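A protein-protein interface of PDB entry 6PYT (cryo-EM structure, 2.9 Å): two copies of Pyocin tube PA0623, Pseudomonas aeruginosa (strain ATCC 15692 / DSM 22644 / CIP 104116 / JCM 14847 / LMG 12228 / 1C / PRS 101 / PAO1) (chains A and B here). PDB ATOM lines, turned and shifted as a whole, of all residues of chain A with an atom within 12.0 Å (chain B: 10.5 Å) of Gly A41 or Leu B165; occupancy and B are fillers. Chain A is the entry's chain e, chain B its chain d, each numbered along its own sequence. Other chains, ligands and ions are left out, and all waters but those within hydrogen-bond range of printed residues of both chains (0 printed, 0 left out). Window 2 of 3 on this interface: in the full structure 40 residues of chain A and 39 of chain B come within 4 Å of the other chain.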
ATOM      1  N   TYR A  37       4.437  -1.429 -15.900  1.00  0.00           N
ATOM      2  CA  TYR A  37       5.027  -1.890 -17.150  1.00  0.00           C
ATOM      3  C   TYR A  37       4.141  -2.953 -17.784  1.00  0.00           C
ATOM      4  O   TYR A  37       4.170  -4.117 -17.385  1.00  0.00           O
ATOM      5  CB  TYR A  37       6.426  -2.436 -16.919  1.00  0.00           C
ATOM      6  CG  TYR A  37       7.113  -2.735 -18.212  1.00  0.00           C
ATOM      7  CD1 TYR A  37       7.639  -1.713 -18.964  1.00  0.00           C
ATOM      8  CD2 TYR A  37       7.197  -4.026 -18.703  1.00  0.00           C
ATOM      9  CE1 TYR A  37       8.247  -1.961 -20.145  1.00  0.00           C
ATOM     10  CE2 TYR A  37       7.806  -4.280 -19.891  1.00  0.00           C
ATOM     11  CZ  TYR A  37       8.328  -3.240 -20.607  1.00  0.00           C
ATOM     12  OH  TYR A  37       8.946  -3.470 -21.801  1.00  0.00           O
ATOM     13  N   ARG A  38       3.393  -2.551 -18.800  1.00  0.00           N
ATOM     14  CA  ARG A  38       2.571  -3.431 -19.617  1.00  0.00           C
ATOM     15  C   ARG A  38       3.161  -3.462 -21.018  1.00  0.00           C
ATOM     16  O   ARG A  38       3.408  -2.410 -21.612  1.00  0.00           O
ATOM     17  CB  ARG A  38       1.132  -2.919 -19.644  1.00  0.00           C
ATOM     18  CG  ARG A  38       0.167  -3.570 -20.607  1.00  0.00           C
ATOM     19  CD  ARG A  38      -0.370  -4.888 -20.149  1.00  0.00           C
ATOM     20  NE  ARG A  38      -1.406  -5.363 -21.064  1.00  0.00           N
ATOM     21  CZ  ARG A  38      -2.694  -5.061 -20.949  1.00  0.00           C
ATOM     22  NH1 ARG A  38      -3.103  -4.291 -19.959  1.00  0.00           N
ATOM     23  NH2 ARG A  38      -3.575  -5.531 -21.819  1.00  0.00           N
ATOM     24  N   ALA A  39       3.386  -4.657 -21.544  1.00  0.00           N
ATOM     25  CA  ALA A  39       4.068  -4.800 -22.821  1.00  0.00           C
ATOM     26  C   ALA A  39       3.502  -6.016 -23.535  1.00  0.00           C
ATOM     27  O   ALA A  39       2.369  -6.429 -23.275  1.00  0.00           O
ATOM     28  CB  ALA A  39       5.588  -4.891 -22.633  1.00  0.00           C
ATOM     29  N   GLY A  40       4.284  -6.566 -24.460  1.00  0.00           N
ATOM     30  CA  GLY A  40       3.779  -7.606 -25.330  1.00  0.00           C
ATOM     31  C   GLY A  40       3.571  -8.912 -24.592  1.00  0.00           C
ATOM     32  O   GLY A  40       4.337  -9.276 -23.704  1.00  0.00           O
ATOM     33  N   GLY A  41       2.497  -9.604 -24.948  1.00  0.00           N
ATOM     34  CA  GLY A  41       2.239 -10.917 -24.402  1.00  0.00           C
ATOM     35  C   GLY A  41       1.821 -10.944 -22.954  1.00  0.00           C
ATOM     36  O   GLY A  41       2.058 -11.947 -22.274  1.00  0.00           O
ATOM     37  N   MET A  42       1.203  -9.879 -22.456  1.00  0.00           N
ATOM     38  CA  MET A  42       0.797  -9.853 -21.060  1.00  0.00           C
ATOM     39  C   MET A  42      -0.377  -8.914 -20.848  1.00  0.00           C
ATOM     40  O   MET A  42      -0.472  -7.871 -21.491  1.00  0.00           O
ATOM     41  CB  MET A  42       1.973  -9.487 -20.149  1.00  0.00           C
ATOM     42  CG  MET A  42       2.722  -8.220 -20.387  1.00  0.00           C
ATOM     43  SD  MET A  42       4.010  -8.259 -19.128  1.00  0.00           S
ATOM     44  CE  MET A  42       4.976  -6.828 -19.514  1.00  0.00           C
ATOM     45  N   ASP A  43      -1.274  -9.309 -19.941  1.00  0.00           N
ATOM     46  CA  ASP A  43      -2.537  -8.621 -19.712  1.00  0.00           C
ATOM     47  C   ASP A  43      -2.497  -7.628 -18.564  1.00  0.00           C
ATOM     48  O   ASP A  43      -3.456  -6.874 -18.395  1.00  0.00           O
ATOM     49  CB  ASP A  43      -3.656  -9.621 -19.421  1.00  0.00           C
ATOM     50  N   ALA A  44      -1.447  -7.627 -17.756  1.00  0.00           N
ATOM     51  CA  ALA A  44      -1.405  -6.785 -16.577  1.00  0.00           C
ATOM     52  C   ALA A  44      -0.030  -6.153 -16.457  1.00  0.00           C
ATOM     53  O   ALA A  44       0.963  -6.736 -16.907  1.00  0.00           O
ATOM     54  CB  ALA A  44      -1.726  -7.595 -15.313  1.00  0.00           C
ATOM     55  N   PRO A  45       0.061  -4.960 -15.872  1.00  0.00           N
ATOM     56  CA  PRO A  45       1.371  -4.351 -15.624  1.00  0.00           C
ATOM     57  C   PRO A  45       2.128  -5.087 -14.530  1.00  0.00           C
ATOM     58  O   PRO A  45       1.588  -5.937 -13.824  1.00  0.00           O
ATOM     59  CB  PRO A  45       1.021  -2.924 -15.204  1.00  0.00           C
ATOM     60  CG  PRO A  45      -0.327  -2.692 -15.745  1.00  0.00           C
ATOM     61  CD  PRO A  45      -1.027  -3.997 -15.654  1.00  0.00           C
ATOM     62  N   VAL A  46       3.412  -4.754 -14.390  1.00  0.00           N
ATOM     63  CA  VAL A  46       4.270  -5.576 -13.547  1.00  0.00           C
ATOM     64  C   VAL A  46       5.167  -4.737 -12.632  1.00  0.00           C
ATOM     65  O   VAL A  46       5.795  -5.283 -11.717  1.00  0.00           O
ATOM     66  CB  VAL A  46       5.088  -6.542 -14.426  1.00  0.00           C
ATOM     67  CG1 VAL A  46       6.304  -5.861 -15.022  1.00  0.00           C
ATOM     68  CG2 VAL A  46       5.419  -7.832 -13.694  1.00  0.00           C
ATOM     69  N   MET B  50      -9.796  -4.722 -21.710  1.00  0.00           N
ATOM     70  CA  MET B  50      -8.506  -4.432 -22.322  1.00  0.00           C
ATOM     71  C   MET B  50      -7.362  -5.030 -21.513  1.00  0.00           C
ATOM     72  O   MET B  50      -6.219  -4.601 -21.663  1.00  0.00           O
ATOM     73  CB  MET B  50      -8.300  -2.922 -22.459  1.00  0.00           C
ATOM     74  CG  MET B  50      -9.401  -2.183 -23.199  1.00  0.00           C
ATOM     75  SD  MET B  50      -9.555  -2.705 -24.897  1.00  0.00           S
ATOM     76  CE  MET B  50      -8.071  -1.961 -25.525  1.00  0.00           C
ATOM     77  N   GLY B  51      -7.648  -5.993 -20.650  1.00  0.00           N
ATOM     78  CA  GLY B  51      -6.668  -6.549 -19.737  1.00  0.00           C
ATOM     79  C   GLY B  51      -6.926  -6.096 -18.313  1.00  0.00           C
ATOM     80  O   GLY B  51      -7.842  -5.326 -18.032  1.00  0.00           O
ATOM     81  N   ASP B 144      -0.827 -14.024 -13.221  1.00  0.00           N
ATOM     82  CA  ASP B 144       0.612 -13.920 -13.426  1.00  0.00           C
ATOM     83  C   ASP B 144       0.783 -13.119 -14.707  1.00  0.00           C
ATOM     84  O   ASP B 144       0.553 -13.661 -15.800  1.00  0.00           O
ATOM     85  CB  ASP B 144       1.246 -15.297 -13.532  1.00  0.00           C
ATOM     86  N   PRO B 145       1.120 -11.817 -14.609  1.00  0.00           N
ATOM     87  CA  PRO B 145       1.223 -10.966 -15.803  1.00  0.00           C
ATOM     88  C   PRO B 145       2.248 -11.433 -16.817  1.00  0.00           C
ATOM     89  O   PRO B 145       1.870 -11.796 -17.928  1.00  0.00           O
ATOM     90  CB  PRO B 145       1.612  -9.607 -15.217  1.00  0.00           C
ATOM     91  CG  PRO B 145       1.098  -9.639 -13.846  1.00  0.00           C
ATOM     92  CD  PRO B 145       1.270 -11.034 -13.378  1.00  0.00           C
ATOM     93  N   VAL B 146       3.526 -11.489 -16.446  1.00  0.00           N
ATOM     94  CA  VAL B 146       4.490 -12.210 -17.260  1.00  0.00           C
ATOM     95  C   VAL B 146       4.149 -13.688 -17.151  1.00  0.00           C
ATOM     96  O   VAL B 146       3.720 -14.141 -16.084  1.00  0.00           O
ATOM     97  CB  VAL B 146       5.917 -11.905 -16.778  1.00  0.00           C
ATOM     98  CG1 VAL B 146       6.944 -12.465 -17.734  1.00  0.00           C
ATOM     99  CG2 VAL B 146       6.097 -10.418 -16.588  1.00  0.00           C
ATOM    100  N   ASN B 147       4.303 -14.432 -18.252  1.00  0.00           N
ATOM    101  CA  ASN B 147       3.638 -15.723 -18.470  1.00  0.00           C
ATOM    102  C   ASN B 147       2.131 -15.556 -18.300  1.00  0.00           C
ATOM    103  O   ASN B 147       1.557 -16.005 -17.316  1.00  0.00           O
ATOM    104  CB  ASN B 147       4.120 -16.851 -17.546  1.00  0.00           C
ATOM    105  CG  ASN B 147       5.507 -17.316 -17.854  1.00  0.00           C
ATOM    106  OD1 ASN B 147       5.890 -17.462 -19.013  1.00  0.00           O
ATOM    107  ND2 ASN B 147       6.272 -17.578 -16.807  1.00  0.00           N
ATOM    108  N   GLY B 148       1.532 -14.835 -19.250  1.00  0.00           N
ATOM    109  CA  GLY B 148       0.187 -14.313 -19.101  1.00  0.00           C
ATOM    110  C   GLY B 148      -0.910 -15.314 -18.815  1.00  0.00           C
ATOM    111  O   GLY B 148      -1.424 -15.986 -19.710  1.00  0.00           O
ATOM    112  N   VAL B 149      -1.299 -15.366 -17.546  1.00  0.00           N
ATOM    113  CA  VAL B 149      -2.249 -16.327 -17.011  1.00  0.00           C
ATOM    114  C   VAL B 149      -3.301 -15.552 -16.241  1.00  0.00           C
ATOM    115  O   VAL B 149      -2.964 -14.741 -15.374  1.00  0.00           O
ATOM    116  CB  VAL B 149      -1.559 -17.357 -16.092  1.00  0.00           C
ATOM    117  CG1 VAL B 149      -2.575 -18.161 -15.308  1.00  0.00           C
ATOM    118  CG2 VAL B 149      -0.702 -18.301 -16.897  1.00  0.00           C
ATOM    119  N   ARG B 150      -4.569 -15.787 -16.560  1.00  0.00           N
ATOM    120  CA  ARG B 150      -5.677 -15.243 -15.785  1.00  0.00           C
ATOM    121  C   ARG B 150      -6.683 -16.371 -15.590  1.00  0.00           C
ATOM    122  O   ARG B 150      -7.605 -16.533 -16.388  1.00  0.00           O
ATOM    123  CB  ARG B 150      -6.281 -14.036 -16.478  1.00  0.00           C
ATOM    124  CG  ARG B 150      -7.283 -13.300 -15.641  1.00  0.00           C
ATOM    125  CD  ARG B 150      -7.745 -12.029 -16.307  1.00  0.00           C
ATOM    126  NE  ARG B 150      -8.581 -12.264 -17.473  1.00  0.00           N
ATOM    127  CZ  ARG B 150      -8.983 -11.302 -18.294  1.00  0.00           C
ATOM    128  NH1 ARG B 150      -8.617 -10.052 -18.070  1.00  0.00           N
ATOM    129  NH2 ARG B 150      -9.750 -11.587 -19.336  1.00  0.00           N
ATOM    130  N   LEU B 158      -6.918 -16.653 -20.630  1.00  0.00           N
ATOM    131  CA  LEU B 158      -6.029 -16.128 -21.647  1.00  0.00           C
ATOM    132  C   LEU B 158      -5.473 -17.197 -22.566  1.00  0.00           C
ATOM    133  O   LEU B 158      -4.442 -16.963 -23.194  1.00  0.00           O
ATOM    134  CB  LEU B 158      -4.870 -15.385 -21.005  1.00  0.00           C
ATOM    135  CG  LEU B 158      -5.197 -14.159 -20.174  1.00  0.00           C
ATOM    136  CD1 LEU B 158      -3.905 -13.632 -19.678  1.00  0.00           C
ATOM    137  CD2 LEU B 158      -5.940 -13.113 -20.966  1.00  0.00           C
ATOM    138  N   ALA B 159      -6.113 -18.360 -22.660  1.00  0.00           N
ATOM    139  CA  ALA B 159      -5.706 -19.342 -23.657  1.00  0.00           C
ATOM    140  C   ALA B 159      -6.063 -18.878 -25.062  1.00  0.00           C
ATOM    141  O   ALA B 159      -5.472 -19.337 -26.044  1.00  0.00           O
ATOM    142  CB  ALA B 159      -6.356 -20.691 -23.365  1.00  0.00           C
ATOM    143  N   GLY B 160      -7.040 -17.977 -25.174  1.00  0.00           N
ATOM    144  CA  GLY B 160      -7.375 -17.422 -26.473  1.00  0.00           C
ATOM    145  C   GLY B 160      -6.276 -16.537 -27.026  1.00  0.00           C
ATOM    146  O   GLY B 160      -5.831 -16.722 -28.159  1.00  0.00           O
ATOM    147  N   MET B 161      -5.811 -15.573 -26.226  1.00  0.00           N
ATOM    148  CA  MET B 161      -4.737 -14.698 -26.675  1.00  0.00           C
ATOM    149  C   MET B 161      -3.389 -15.394 -26.708  1.00  0.00           C
ATOM    150  O   MET B 161      -2.473 -14.900 -27.365  1.00  0.00           O
ATOM    151  CB  MET B 161      -4.650 -13.445 -25.798  1.00  0.00           C
ATOM    152  CG  MET B 161      -4.456 -13.691 -24.308  1.00  0.00           C
ATOM    153  SD  MET B 161      -2.788 -14.016 -23.674  1.00  0.00           S
ATOM    154  CE  MET B 161      -2.032 -12.405 -23.714  1.00  0.00           C
ATOM    155  N   ARG B 162      -3.234 -16.507 -25.996  1.00  0.00           N
ATOM    156  CA  ARG B 162      -1.940 -17.175 -25.947  1.00  0.00           C
ATOM    157  C   ARG B 162      -1.615 -17.846 -27.271  1.00  0.00           C
ATOM    158  O   ARG B 162      -0.473 -17.794 -27.734  1.00  0.00           O
ATOM    159  CB  ARG B 162      -1.929 -18.199 -24.823  1.00  0.00           C
ATOM    160  CG  ARG B 162      -0.595 -18.831 -24.579  1.00  0.00           C
ATOM    161  CD  ARG B 162      -0.714 -19.877 -23.504  1.00  0.00           C
ATOM    162  NE  ARG B 162      -1.145 -19.279 -22.252  1.00  0.00           N
ATOM    163  CZ  ARG B 162      -0.321 -18.708 -21.390  1.00  0.00           C
ATOM    164  NH1 ARG B 162       0.982 -18.663 -21.632  1.00  0.00           N
ATOM    165  NH2 ARG B 162      -0.800 -18.190 -20.277  1.00  0.00           N
ATOM    166  N   ASN B 163      -2.606 -18.478 -27.893  1.00  0.00           N
ATOM    167  CA  ASN B 163      -2.398 -19.075 -29.203  1.00  0.00           C
ATOM    168  C   ASN B 163      -2.352 -18.032 -30.304  1.00  0.00           C
ATOM    169  O   ASN B 163      -1.711 -18.257 -31.334  1.00  0.00           O
ATOM    170  CB  ASN B 163      -3.497 -20.089 -29.496  1.00  0.00           C
ATOM    171  CG  ASN B 163      -3.372 -21.328 -28.654  1.00  0.00           C
ATOM    172  OD1 ASN B 163      -2.274 -21.848 -28.458  1.00  0.00           O
ATOM    173  ND2 ASN B 163      -4.494 -21.812 -28.142  1.00  0.00           N
ATOM    174  N   ASP B 164      -3.028 -16.899 -30.113  1.00  0.00           N
ATOM    175  CA  ASP B 164      -2.992 -15.842 -31.114  1.00  0.00           C
ATOM    176  C   ASP B 164      -1.623 -15.190 -31.168  1.00  0.00           C
ATOM    177  O   ASP B 164      -1.119 -14.878 -32.252  1.00  0.00           O
ATOM    178  CB  ASP B 164      -4.055 -14.794 -30.814  1.00  0.00           C
ATOM    179  N   LEU B 165      -1.004 -14.987 -30.015  1.00  0.00           N
ATOM    180  CA  LEU B 165       0.301 -14.362 -29.964  1.00  0.00           C
ATOM    181  C   LEU B 165       1.436 -15.354 -30.138  1.00  0.00           C
ATOM    182  O   LEU B 165       2.588 -14.931 -30.240  1.00  0.00           O
ATOM    183  CB  LEU B 165       0.479 -13.622 -28.642  1.00  0.00           C
ATOM    184  CG  LEU B 165      -0.497 -12.483 -28.397  1.00  0.00           C
ATOM    185  CD1 LEU B 165      -0.214 -11.850 -27.058  1.00  0.00           C
ATOM    186  CD2 LEU B 165      -0.450 -11.464 -29.504  1.00  0.00           C
ATOM    187  N   GLY B 166       1.141 -16.648 -30.174  1.00  0.00           N
ATOM    188  CA  GLY B 166       2.181 -17.647 -30.280  1.00  0.00           C
ATOM    189  C   GLY B 166       3.042 -17.759 -29.049  1.00  0.00           C
ATOM    190  O   GLY B 166       4.238 -18.026 -29.161  1.00  0.00           O
ATOM    191  N   LEU B 167       2.462 -17.560 -27.874  1.00  0.00           N
ATOM    192  CA  LEU B 167       3.224 -17.506 -26.638  1.00  0.00           C
ATOM    193  C   LEU B 167       3.616 -18.884 -26.139  1.00  0.00           C
ATOM    194  O   LEU B 167       4.469 -19.553 -26.714  1.00  0.00           O
ATOM    195  CB  LEU B 167       2.428 -16.783 -25.558  1.00  0.00           C
ATOM    196  CG  LEU B 167       2.200 -15.296 -25.773  1.00  0.00           C
ATOM    197  CD1 LEU B 167       1.284 -14.736 -24.707  1.00  0.00           C
ATOM    198  CD2 LEU B 167       3.524 -14.603 -25.741  1.00  0.00           C
ATOM    199  OXT LEU B 167       3.100 -19.353 -25.128  1.00  0.00           O
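NH2 of Arg A38 is in hydrogen-bond range of O of Met B50, at 2.8 Å.
N of Leu B167 sits at hydrogen-bond distance from O of Arg B162, 2.9 Å away. The backbone carbonyl oxygen of Tyr A37 lies within hydrogen-bond range of the backbone NH of Val A46, at 3.2 Å. The guanidinium group (NH1) of Arg A38 is in hydrogen-bond range of the backbone carbonyl oxygen (O) of Asp A43, at 3.0 Å. NE of Arg A38 sits at hydrogen-bond distance from O of Met A42 (2.7 Å).
CA of Gly B51 touches NH2 of Arg A38 (3.9 Å). Gly A41 touches Leu B165 (CA to CD1, 3.7 Å). CD1 of Leu B167 touches O of Gly A41, at 3.8 Å. Met A42 touches Pro B145 (CB to O, 3.2 Å). Met A42 touches Val B146 (SD to CG2, 3.9 Å). Asp A43 touches Gly B51. Ala A44 touches Pro B145 (O to CB, 3.4 Å). CG of Pro B145 touches O of Pro A45, at 3.7 Å. Val B146 touches Val A46.
Tyr A37 touches none of the printed residues of chain B. Ala A39 touches none of the printed residues of chain B. No residue of chain B comes within 4 Å of Gly A40. Of chain B, only Leu B165 (3.7 Å) and Leu B167 (3.8 Å) come within 4 Å of Gly A41. Of the printed residues of chain B, Asp A43 touches Gly B51. Of the printed residues of chain B, Ala A44 touches Pro B145. Of the printed residues of chain B, Pro A45 touches Pro B145. Printed residues of chain A within 4 Å of Val B146: Met A42 (3.9 Å) and Val A46 (3.9 Å). No residue of chain A comes within 4 Å of Gly B148. No residue of chain A comes within 4 Å of Met B161. Asn B163 touches none of the printed residues of chain A. No residue of chain A comes within 4 Å of Asp B164. Of chain A, only Gly A41 comes within 4 Å of Leu B165. No residue of chain A comes within 4 Å of Gly B166. The nearest printed residue of chain B that does not touch Gly A41 is Met B161 (4.2 Å). The nearest residue of chain A that does not touch Leu B165 is Met A42 (5.2 Å).
Hydrophobic or aromatic side chains of chain A that line the printed part of chain B: Met A42, Ala A44 and Val A46. Hydrophobic or aromatic side chains of chain B that line the printed part of chain A: Pro B145, Val B146, Leu B165 and Leu B167.
No position is printed for both chains.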
